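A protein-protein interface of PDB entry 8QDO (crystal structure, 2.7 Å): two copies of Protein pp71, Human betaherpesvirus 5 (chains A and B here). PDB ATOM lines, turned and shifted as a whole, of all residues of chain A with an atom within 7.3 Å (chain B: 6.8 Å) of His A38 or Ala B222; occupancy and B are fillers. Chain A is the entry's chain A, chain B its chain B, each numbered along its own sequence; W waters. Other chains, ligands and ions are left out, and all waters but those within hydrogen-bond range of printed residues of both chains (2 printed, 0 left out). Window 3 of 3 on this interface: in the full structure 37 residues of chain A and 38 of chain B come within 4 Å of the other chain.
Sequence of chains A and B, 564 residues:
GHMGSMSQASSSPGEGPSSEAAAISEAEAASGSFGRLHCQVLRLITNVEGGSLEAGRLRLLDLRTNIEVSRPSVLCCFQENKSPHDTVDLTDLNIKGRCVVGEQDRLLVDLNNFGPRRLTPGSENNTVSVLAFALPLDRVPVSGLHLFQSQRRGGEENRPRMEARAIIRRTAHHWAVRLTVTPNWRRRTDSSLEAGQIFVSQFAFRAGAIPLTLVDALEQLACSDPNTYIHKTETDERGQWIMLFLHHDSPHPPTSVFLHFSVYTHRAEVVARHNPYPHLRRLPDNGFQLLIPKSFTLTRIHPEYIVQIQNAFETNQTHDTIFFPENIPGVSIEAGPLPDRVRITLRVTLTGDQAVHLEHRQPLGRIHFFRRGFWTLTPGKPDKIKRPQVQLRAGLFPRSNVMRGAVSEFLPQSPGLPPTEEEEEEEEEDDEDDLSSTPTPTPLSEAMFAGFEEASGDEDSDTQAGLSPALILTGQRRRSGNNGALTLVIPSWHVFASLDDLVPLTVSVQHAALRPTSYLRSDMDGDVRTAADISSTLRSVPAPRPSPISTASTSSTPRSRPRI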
ATOM      1  N   ALA A  29      23.876  36.875  13.031  1.00  0.00           N
ATOM      2  CA  ALA A  29      24.604  35.613  13.118  1.00  0.00           C
ATOM      3  C   ALA A  29      25.120  35.385  14.534  1.00  0.00           C
ATOM      4  O   ALA A  29      24.996  34.282  15.083  1.00  0.00           O
ATOM      5  CB  ALA A  29      25.752  35.605  12.110  1.00  0.00           C
ATOM      6  N   ALA A  30      25.651  36.438  15.162  1.00  0.00           N
ATOM      7  CA  ALA A  30      26.218  36.308  16.497  1.00  0.00           C
ATOM      8  C   ALA A  30      25.136  36.084  17.547  1.00  0.00           C
ATOM      9  O   ALA A  30      25.332  35.311  18.493  1.00  0.00           O
ATOM     10  CB  ALA A  30      27.044  37.551  16.832  1.00  0.00           C
ATOM     11  N   SER A  31      23.987  36.736  17.405  1.00  0.00           N
ATOM     12  CA  SER A  31      22.985  36.665  18.463  1.00  0.00           C
ATOM     13  C   SER A  31      22.131  35.402  18.399  1.00  0.00           C
ATOM     14  O   SER A  31      21.432  35.100  19.369  1.00  0.00           O
ATOM     15  CB  SER A  31      22.087  37.901  18.431  1.00  0.00           C
ATOM     16  OG  SER A  31      21.259  37.850  17.291  1.00  0.00           O
ATOM     17  N   GLY A  32      22.126  34.694  17.281  1.00  0.00           N
ATOM     18  CA  GLY A  32      21.451  33.416  17.209  1.00  0.00           C
ATOM     19  C   GLY A  32      19.931  33.496  17.273  1.00  0.00           C
ATOM     20  O   GLY A  32      19.308  34.554  17.205  1.00  0.00           O
ATOM     21  N   SER A  33      19.341  32.312  17.370  1.00  0.00           N
ATOM     22  CA  SER A  33      17.902  32.155  17.493  1.00  0.00           C
ATOM     23  C   SER A  33      17.641  30.843  18.221  1.00  0.00           C
ATOM     24  O   SER A  33      18.570  30.116  18.578  1.00  0.00           O
ATOM     25  CB  SER A  33      17.225  32.176  16.126  1.00  0.00           C
ATOM     26  OG  SER A  33      17.594  31.019  15.394  1.00  0.00           O
ATOM     27  N   ARG A  36      19.477  27.816  16.940  1.00  0.00           N
ATOM     28  CA  ARG A  36      20.920  27.775  17.097  1.00  0.00           C
ATOM     29  C   ARG A  36      21.415  29.042  17.779  1.00  0.00           C
ATOM     30  O   ARG A  36      21.338  30.131  17.204  1.00  0.00           O
ATOM     31  CB  ARG A  36      21.588  27.585  15.734  1.00  0.00           C
ATOM     32  CG  ARG A  36      23.079  27.330  15.804  1.00  0.00           C
ATOM     33  CD  ARG A  36      23.633  27.008  14.439  1.00  0.00           C
ATOM     34  NE  ARG A  36      25.049  26.663  14.440  1.00  0.00           N
ATOM     35  CZ  ARG A  36      25.530  25.455  14.706  1.00  0.00           C
ATOM     36  NH1 ARG A  36      24.735  24.454  15.051  1.00  0.00           N
ATOM     37  NH2 ARG A  36      26.838  25.240  14.607  1.00  0.00           N
ATOM     38  N   LEU A  37      21.894  28.924  19.012  1.00  0.00           N
ATOM     39  CA  LEU A  37      22.413  30.073  19.737  1.00  0.00           C
ATOM     40  C   LEU A  37      23.668  29.641  20.488  1.00  0.00           C
ATOM     41  O   LEU A  37      24.003  28.454  20.568  1.00  0.00           O
ATOM     42  CB  LEU A  37      21.364  30.710  20.660  1.00  0.00           C
ATOM     43  CG  LEU A  37      20.805  29.991  21.880  1.00  0.00           C
ATOM     44  CD1 LEU A  37      21.862  29.856  22.978  1.00  0.00           C
ATOM     45  CD2 LEU A  37      19.578  30.757  22.368  1.00  0.00           C
ATOM     46  N   HIS A  38      24.378  30.628  21.018  1.00  0.00           N
ATOM     47  CA  HIS A  38      25.659  30.406  21.663  1.00  0.00           C
ATOM     48  C   HIS A  38      25.712  31.157  22.977  1.00  0.00           C
ATOM     49  O   HIS A  38      25.273  32.303  23.061  1.00  0.00           O
ATOM     50  CB  HIS A  38      26.798  30.854  20.752  1.00  0.00           C
ATOM     51  CG  HIS A  38      26.700  30.295  19.369  1.00  0.00           C
ATOM     52  ND1 HIS A  38      26.936  28.966  19.086  1.00  0.00           N
ATOM     53  CD2 HIS A  38      26.365  30.874  18.194  1.00  0.00           C
ATOM     54  CE1 HIS A  38      26.770  28.755  17.793  1.00  0.00           C
ATOM     55  NE2 HIS A  38      26.422  29.898  17.228  1.00  0.00           N
ATOM     56  N   CYS A  39      26.230  30.497  24.004  1.00  0.00           N
ATOM     57  CA  CYS A  39      26.326  31.111  25.319  1.00  0.00           C
ATOM     58  C   CYS A  39      27.249  30.250  26.167  1.00  0.00           C
ATOM     59  O   CYS A  39      27.556  29.107  25.816  1.00  0.00           O
ATOM     60  CB  CYS A  39      24.955  31.243  25.968  1.00  0.00           C
ATOM     61  SG  CYS A  39      24.132  29.654  26.133  1.00  0.00           S
ATOM     62  N   GLN A  40      27.686  30.819  27.295  1.00  0.00           N
ATOM     63  CA  GLN A  40      28.435  30.090  28.313  1.00  0.00           C
ATOM     64  C   GLN A  40      27.505  29.370  29.279  1.00  0.00           C
ATOM     65  O   GLN A  40      27.785  28.239  29.692  1.00  0.00           O
ATOM     66  CB  GLN A  40      29.348  31.049  29.087  1.00  0.00           C
ATOM     67  CG  GLN A  40      30.370  31.755  28.235  1.00  0.00           C
ATOM     68  CD  GLN A  40      31.298  30.780  27.531  1.00  0.00           C
ATOM     69  OE1 GLN A  40      31.096  30.433  26.363  1.00  0.00           O
ATOM     70  NE2 GLN A  40      32.336  30.348  28.234  1.00  0.00           N
ATOM     71  N   VAL A  41      26.398  30.008  29.649  1.00  0.00           N
ATOM     72  CA  VAL A  41      25.376  29.400  30.487  1.00  0.00           C
ATOM     73  C   VAL A  41      24.033  29.640  29.814  1.00  0.00           C
ATOM     74  O   VAL A  41      23.750  30.758  29.370  1.00  0.00           O
ATOM     75  CB  VAL A  41      25.378  29.967  31.921  1.00  0.00           C
ATOM     76  CG1 VAL A  41      24.229  29.364  32.732  1.00  0.00           C
ATOM     77  CG2 VAL A  41      26.721  29.715  32.601  1.00  0.00           C
ATOM     78  N   GLU A  68      25.333  21.284  22.420  1.00  0.00           N
ATOM     79  CA  GLU A  68      26.483  20.800  21.675  1.00  0.00           C
ATOM     80  C   GLU A  68      27.724  21.571  22.095  1.00  0.00           C
ATOM     81  O   GLU A  68      27.653  22.764  22.406  1.00  0.00           O
ATOM     82  CB  GLU A  68      26.290  20.946  20.170  1.00  0.00           C
ATOM     83  CG  GLU A  68      25.265  20.026  19.553  1.00  0.00           C
ATOM     84  CD  GLU A  68      25.389  19.980  18.037  1.00  0.00           C
ATOM     85  OE1 GLU A  68      26.122  20.831  17.470  1.00  0.00           O
ATOM     86  OE2 GLU A  68      24.755  19.096  17.417  1.00  0.00           O
ATOM     87  N   SER A  70      32.244  21.536  21.109  1.00  0.00           N
ATOM     88  CA  SER A  70      33.162  21.113  20.062  1.00  0.00           C
ATOM     89  C   SER A  70      34.287  20.218  20.565  1.00  0.00           C
ATOM     90  O   SER A  70      35.095  19.750  19.758  1.00  0.00           O
ATOM     91  CB  SER A  70      33.742  22.344  19.372  1.00  0.00           C
ATOM     92  OG  SER A  70      34.665  22.983  20.233  1.00  0.00           O
ATOM     93  N   PRO A 504      32.124  26.845  25.521  1.00  0.00           N
ATOM     94  CA  PRO A 504      31.012  27.519  24.827  1.00  0.00           C
ATOM     95  C   PRO A 504      29.975  26.536  24.301  1.00  0.00           C
ATOM     96  O   PRO A 504      30.306  25.567  23.611  1.00  0.00           O
ATOM     97  CB  PRO A 504      31.712  28.260  23.685  1.00  0.00           C
ATOM     98  CG  PRO A 504      33.119  28.496  24.213  1.00  0.00           C
ATOM     99  CD  PRO A 504      33.441  27.264  25.007  1.00  0.00           C
ATOM    100  N   LEU A 505      28.706  26.810  24.622  1.00  0.00           N
ATOM    101  CA  LEU A 505      27.585  25.967  24.226  1.00  0.00           C
ATOM    102  C   LEU A 505      26.999  26.383  22.888  1.00  0.00           C
ATOM    103  O   LEU A 505      26.965  27.566  22.537  1.00  0.00           O
ATOM    104  CB  LEU A 505      26.453  26.011  25.251  1.00  0.00           C
ATOM    105  CG  LEU A 505      26.664  25.545  26.679  1.00  0.00           C
ATOM    106  CD1 LEU A 505      25.310  25.545  27.361  1.00  0.00           C
ATOM    107  CD2 LEU A 505      27.298  24.168  26.695  1.00  0.00           C
ATOM    108  N   THR A 506      26.501  25.389  22.158  1.00  0.00           N
ATOM    109  CA  THR A 506      25.672  25.587  20.974  1.00  0.00           C
ATOM    110  C   THR A 506      24.310  24.993  21.274  1.00  0.00           C
ATOM    111  O   THR A 506      24.158  23.768  21.330  1.00  0.00           O
ATOM    112  CB  THR A 506      26.286  24.937  19.746  1.00  0.00           C
ATOM    113  OG1 THR A 506      27.384  25.742  19.289  1.00  0.00           O
ATOM    114  CG2 THR A 506      25.240  24.771  18.651  1.00  0.00           C
ATOM    115  N   VAL A 507      23.336  25.852  21.496  1.00  0.00           N
ATOM    116  CA  VAL A 507      22.023  25.433  21.953  1.00  0.00           C
ATOM    117  C   VAL A 507      21.077  25.336  20.765  1.00  0.00           C
ATOM    118  O   VAL A 507      21.127  26.155  19.839  1.00  0.00           O
ATOM    119  CB  VAL A 507      21.479  26.407  23.011  1.00  0.00           C
ATOM    120  CG1 VAL A 507      20.089  25.952  23.469  1.00  0.00           C
ATOM    121  CG2 VAL A 507      22.429  26.471  24.170  1.00  0.00           C
ATOM    122  N   SER A 522      19.263  38.021  26.960  1.00  0.00           N
ATOM    123  CA  SER A 522      20.713  38.034  26.907  1.00  0.00           C
ATOM    124  C   SER A 522      21.267  38.842  28.068  1.00  0.00           C
ATOM    125  O   SER A 522      20.749  39.912  28.399  1.00  0.00           O
ATOM    126  CB  SER A 522      21.228  38.604  25.595  1.00  0.00           C
ATOM    127  OG  SER A 522      22.637  38.499  25.560  1.00  0.00           O
ATOM    128  N   GLY A 526      25.987  38.503  26.100  1.00  0.00           N
ATOM    129  CA  GLY A 526      25.742  37.264  25.402  1.00  0.00           C
ATOM    130  C   GLY A 526      26.313  36.024  26.052  1.00  0.00           C
ATOM    131  O   GLY A 526      26.166  34.934  25.487  1.00  0.00           O
ATOM    132  N   ASP A 527      26.967  36.145  27.213  1.00  0.00           N
ATOM    133  CA  ASP A 527      27.475  34.950  27.881  1.00  0.00           C
ATOM    134  C   ASP A 527      26.355  34.139  28.523  1.00  0.00           C
ATOM    135  O   ASP A 527      26.451  32.908  28.593  1.00  0.00           O
ATOM    136  CB  ASP A 527      28.523  35.329  28.925  1.00  0.00           C
ATOM    137  CG  ASP A 527      29.896  35.608  28.311  1.00  0.00           C
ATOM    138  OD1 ASP A 527      30.073  35.411  27.084  1.00  0.00           O
ATOM    139  OD2 ASP A 527      30.801  36.031  29.067  1.00  0.00           O
ATOM    140  N   VAL A 528      25.281  34.796  28.965  1.00  0.00           N
ATOM    141  CA  VAL A 528      24.117  34.136  29.557  1.00  0.00           C
ATOM    142  C   VAL A 528      22.917  34.387  28.646  1.00  0.00           C
ATOM    143  O   VAL A 528      22.499  35.537  28.467  1.00  0.00           O
ATOM    144  CB  VAL A 528      23.843  34.628  30.986  1.00  0.00           C
ATOM    145  CG1 VAL A 528      22.607  33.953  31.561  1.00  0.00           C
ATOM    146  CG2 VAL A 528      25.038  34.340  31.881  1.00  0.00           C
ATOM    147  N   ARG A 529      22.383  33.324  28.043  1.00  0.00           N
ATOM    148  CA  ARG A 529      21.189  33.405  27.208  1.00  0.00           C
ATOM    149  C   ARG A 529      20.036  32.668  27.871  1.00  0.00           C
ATOM    150  O   ARG A 529      20.211  31.579  28.425  1.00  0.00           O
ATOM    151  CB  ARG A 529      21.413  32.820  25.818  1.00  0.00           C
ATOM    152  CG  ARG A 529      22.535  33.471  25.038  1.00  0.00           C
ATOM    153  CD  ARG A 529      22.352  34.972  24.937  1.00  0.00           C
ATOM    154  NE  ARG A 529      21.084  35.336  24.320  1.00  0.00           N
ATOM    155  CZ  ARG A 529      20.845  35.299  23.016  1.00  0.00           C
ATOM    156  NH1 ARG A 529      21.765  34.892  22.157  1.00  0.00           N
ATOM    157  NH2 ARG A 529      19.653  35.678  22.564  1.00  0.00           N
ATOM    158  N   GLU B 219      41.677  26.855  18.449  1.00  0.00           N
ATOM    159  CA  GLU B 219      40.635  25.845  18.587  1.00  0.00           C
ATOM    160  C   GLU B 219      39.279  26.503  18.388  1.00  0.00           C
ATOM    161  O   GLU B 219      38.935  27.449  19.104  1.00  0.00           O
ATOM    162  CB  GLU B 219      40.694  25.160  19.953  1.00  0.00           C
ATOM    163  CG  GLU B 219      39.743  23.977  20.078  1.00  0.00           C
ATOM    164  CD  GLU B 219      39.946  23.216  21.366  1.00  0.00           C
ATOM    165  OE1 GLU B 219      39.995  23.861  22.438  1.00  0.00           O
ATOM    166  OE2 GLU B 219      40.092  21.977  21.299  1.00  0.00           O
ATOM    167  N   GLN B 220      38.526  26.018  17.405  1.00  0.00           N
ATOM    168  CA  GLN B 220      37.173  26.510  17.181  1.00  0.00           C
ATOM    169  C   GLN B 220      36.241  25.937  18.246  1.00  0.00           C
ATOM    170  O   GLN B 220      36.246  24.726  18.500  1.00  0.00           O
ATOM    171  CB  GLN B 220      36.702  26.128  15.774  1.00  0.00           C
ATOM    172  CG  GLN B 220      35.333  26.662  15.396  1.00  0.00           C
ATOM    173  CD  GLN B 220      34.917  26.293  13.976  1.00  0.00           C
ATOM    174  OE1 GLN B 220      35.734  26.273  13.053  1.00  0.00           O
ATOM    175  NE2 GLN B 220      33.643  25.971  13.807  1.00  0.00           N
ATOM    176  N   LEU B 221      35.455  26.812  18.884  1.00  0.00           N
ATOM    177  CA  LEU B 221      34.541  26.438  19.962  1.00  0.00           C
ATOM    178  C   LEU B 221      33.063  26.610  19.616  1.00  0.00           C
ATOM    179  O   LEU B 221      32.223  25.915  20.195  1.00  0.00           O
ATOM    180  CB  LEU B 221      34.849  27.252  21.225  1.00  0.00           C
ATOM    181  CG  LEU B 221      36.296  27.162  21.727  1.00  0.00           C
ATOM    182  CD1 LEU B 221      36.529  28.131  22.866  1.00  0.00           C
ATOM    183  CD2 LEU B 221      36.658  25.735  22.150  1.00  0.00           C
ATOM    184  N   ALA B 222      32.716  27.519  18.705  1.00  0.00           N
ATOM    185  CA  ALA B 222      31.330  27.697  18.288  1.00  0.00           C
ATOM    186  C   ALA B 222      31.297  28.403  16.940  1.00  0.00           C
ATOM    187  O   ALA B 222      32.188  29.194  16.610  1.00  0.00           O
ATOM    188  CB  ALA B 222      30.514  28.491  19.312  1.00  0.00           C
ATOM    189  N   CYS B 223      30.257  28.105  16.164  1.00  0.00           N
ATOM    190  CA  CYS B 223      30.078  28.744  14.872  1.00  0.00           C
ATOM    191  C   CYS B 223      28.589  28.895  14.594  1.00  0.00           C
ATOM    192  O   CYS B 223      27.801  27.988  14.879  1.00  0.00           O
ATOM    193  CB  CYS B 223      30.753  27.939  13.760  1.00  0.00           C
ATOM    194  SG  CYS B 223      30.679  28.746  12.142  1.00  0.00           S
ATOM    195  N   SER B 224      28.211  30.042  14.022  1.00  0.00           N
ATOM    196  CA  SER B 224      26.803  30.286  13.724  1.00  0.00           C
ATOM    197  C   SER B 224      26.280  29.394  12.612  1.00  0.00           C
ATOM    198  O   SER B 224      25.061  29.265  12.465  1.00  0.00           O
ATOM    199  CB  SER B 224      26.577  31.756  13.362  1.00  0.00           C
ATOM    200  OG  SER B 224      27.375  32.151  12.264  1.00  0.00           O
ATOM    201  N   ASP B 225      27.157  28.750  11.853  1.00  0.00           N
ATOM    202  CA  ASP B 225      26.721  27.863  10.797  1.00  0.00           C
ATOM    203  C   ASP B 225      27.301  26.472  11.019  1.00  0.00           C
ATOM    204  O   ASP B 225      28.513  26.338  11.237  1.00  0.00           O
ATOM    205  CB  ASP B 225      27.141  28.398   9.419  1.00  0.00           C
ATOM    206  CG  ASP B 225      26.774  27.451   8.304  1.00  0.00           C
ATOM    207  OD1 ASP B 225      25.592  27.441   7.879  1.00  0.00           O
ATOM    208  OD2 ASP B 225      27.665  26.689   7.886  1.00  0.00           O
ATOM    209  N   PHE B 258      29.443  34.152  12.457  1.00  0.00           N
ATOM    210  CA  PHE B 258      30.005  34.378  13.779  1.00  0.00           C
ATOM    211  C   PHE B 258      30.916  33.207  14.131  1.00  0.00           C
ATOM    212  O   PHE B 258      30.560  32.044  13.916  1.00  0.00           O
ATOM    213  CB  PHE B 258      28.907  34.506  14.832  1.00  0.00           C
ATOM    214  CG  PHE B 258      29.404  34.339  16.240  1.00  0.00           C
ATOM    215  CD1 PHE B 258      30.044  35.380  16.894  1.00  0.00           C
ATOM    216  CD2 PHE B 258      29.251  33.135  16.901  1.00  0.00           C
ATOM    217  CE1 PHE B 258      30.509  35.226  18.184  1.00  0.00           C
ATOM    218  CE2 PHE B 258      29.714  32.975  18.193  1.00  0.00           C
ATOM    219  CZ  PHE B 258      30.346  34.022  18.832  1.00  0.00           C
ATOM    220  N   LEU B 259      32.099  33.516  14.661  1.00  0.00           N
ATOM    221  CA  LEU B 259      33.058  32.504  15.085  1.00  0.00           C
ATOM    222  C   LEU B 259      33.526  32.804  16.503  1.00  0.00           C
ATOM    223  O   LEU B 259      33.823  33.955  16.847  1.00  0.00           O
ATOM    224  CB  LEU B 259      34.272  32.426  14.148  1.00  0.00           C
ATOM    225  CG  LEU B 259      34.221  31.426  12.994  1.00  0.00           C
ATOM    226  CD1 LEU B 259      35.426  31.604  12.091  1.00  0.00           C
ATOM    227  CD2 LEU B 259      34.165  29.997  13.509  1.00  0.00           C
ATOM    228  N   HIS B 260      33.571  31.756  17.321  1.00  0.00           N
ATOM    229  CA  HIS B 260      34.128  31.788  18.668  1.00  0.00           C
ATOM    230  C   HIS B 260      35.251  30.769  18.700  1.00  0.00           C
ATOM    231  O   HIS B 260      35.005  29.575  18.490  1.00  0.00           O
ATOM    232  CB  HIS B 260      33.057  31.447  19.707  1.00  0.00           C
ATOM    233  CG  HIS B 260      33.462  31.681  21.132  1.00  0.00           C
ATOM    234  ND1 HIS B 260      34.775  31.808  21.537  1.00  0.00           N
ATOM    235  CD2 HIS B 260      32.711  31.813  22.251  1.00  0.00           C
ATOM    236  CE1 HIS B 260      34.813  32.005  22.844  1.00  0.00           C
ATOM    237  NE2 HIS B 260      33.574  32.017  23.300  1.00  0.00           N
ATOM    238  N   PHE B 261      36.482  31.230  18.927  1.00  0.00           N
ATOM    239  CA  PHE B 261      37.613  30.316  18.990  1.00  0.00           C
ATOM    240  C   PHE B 261      38.594  30.785  20.051  1.00  0.00           C
ATOM    241  O   PHE B 261      38.505  31.900  20.569  1.00  0.00           O
ATOM    242  CB  PHE B 261      38.303  30.163  17.621  1.00  0.00           C
ATOM    243  CG  PHE B 261      38.793  31.454  17.023  1.00  0.00           C
ATOM    244  CD1 PHE B 261      37.967  32.221  16.214  1.00  0.00           C
ATOM    245  CD2 PHE B 261      40.097  31.880  17.234  1.00  0.00           C
ATOM    246  CE1 PHE B 261      38.422  33.398  15.645  1.00  0.00           C
ATOM    247  CE2 PHE B 261      40.558  33.056  16.664  1.00  0.00           C
ATOM    248  CZ  PHE B 261      39.722  33.816  15.871  1.00  0.00           C
HETATM  249  O   HOH W   1      29.121  25.834  17.096  1.00  0.00           O
HETATM  250  O   HOH W   2      32.487  24.319  22.394  1.00  0.00           O
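Water W1 lies within hydrogen-bond range of the backbone NH of Cys B223 (2.7 Å), the side-chain hydroxyl of Thr A506 (2.8 Å) and the guanidinium group of Arg A36 (3.4 Å).
Water W2 lies within hydrogen-bond range of the backbone carbonyl oxygen (O) of Leu B221 (2.7 Å), the backbone carbonyl oxygen (O) of Pro A504 (2.8 Å) and the backbone NH (N) of Ser A70 (3.1 Å).
His A38 touches just these residues of chain B: Ala B222 (3.6 Å), Cys B223 (3.2 Å), Ser B224 (3.5 Å) and Phe B258 (3.9 Å).
Of chain A, only His A38 (3.6 Å) comes within 4 Å of Ala B222.
Printed residues of chain A within 4 Å of Leu B221: Ser A70 and Pro A504.
Of the printed residues of chain A, Asp B225 touches Arg A36.
Printed residues of chain B within 4 Å of Ala A29: Ser B224 (3.4 Å) and Phe B258 (3.9 Å).
Of the printed residues of chain A, Gln B220 touches Ser A70 (2.9 Å).
Val A528 touches none of the printed residues of chain B.
Val A41 touches none of the printed residues of chain B.
The nearest residue of chain B that does not touch His A38 is Asp B225 (5.5 Å).
The nearest printed residue of chain A that does not touch Asp B225 is His A38 (5.5 Å).
CB of Ser B224 touches O of Ala A29 (3.4 Å).
C of Ala A29 touches CB of Phe B258, at 3.9 Å.
CB of Phe B258 touches CA of Ala A30, 3.6 Å away.
Asp B225 touches Arg A36.
CB of Ala B222 touches ND1 of His A38 (3.6 Å).
His A38 touches Ser B224 (NE2 to CA, 3.5 Å).
Phe B258 touches His A38.
OG of Ser A70 touches CA of Leu B221 (3.5 Å).
Leu B221 touches Pro A504 (CB to CG, 3.7 Å).
His B260 touches Pro A504.
No position is printed for both chains.
Of the 14 pairs that touch across the chains among the printed residues, none has its exchanged pair printed and touching as well.
The side-chain hydroxyl (OG) of Ser A70 lies within hydrogen-bond range of the backbone carbonyl oxygen (O) of Gln B220, at 2.9 Å.
NE of Arg A36 lies within hydrogen-bond range of O of Ser B224 (3.3 Å).
A ring nitrogen (NE2) of His A38 lies close to the backbone carbonyl oxygen of Cys B223 (3.3 Å).
The backbone carbonyl oxygen (O) of Cys B223 sits at hydrogen-bond distance from the guanidinium group (NH2) of Arg A36 (2.9 Å).
SG of Cys B223 sits close to O of Phe B258, at 3.7 Å.
The backbone NH (N) of Phe B258 sits at hydrogen-bond distance from the side-chain hydroxyl (OG) of Ser B224 (2.9 Å).
The backbone carbonyl oxygen (O) of Ala B222 is in hydrogen-bond range of the backbone NH (N) of His B260 (3.0 Å).
O of Asp B225 is in hydrogen-bond range of SG of Cys B223.
N of Leu B221 lies within hydrogen-bond range of O of His B260 (2.8 Å).
A ring nitrogen (ND1) of His A38 is in hydrogen-bond range of the side-chain hydroxyl (OG1) of Thr A506.
Of the 11 printed residues of chain B, 8 touch a printed residue of chain A.
Printed residues of chain B that touch a printed residue of chain A: Gln B220, Leu B221, Ala B222, Cys B223, Ser B224, Asp B225, Phe B258 and His B260.
Hydrophobic or aromatic side chains of chain A within 4 Å of the printed part of chain B: Ala A29, Ala A30, His A38 and Pro A504.
Among the printed residues, 14 pairs touch across the chains.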
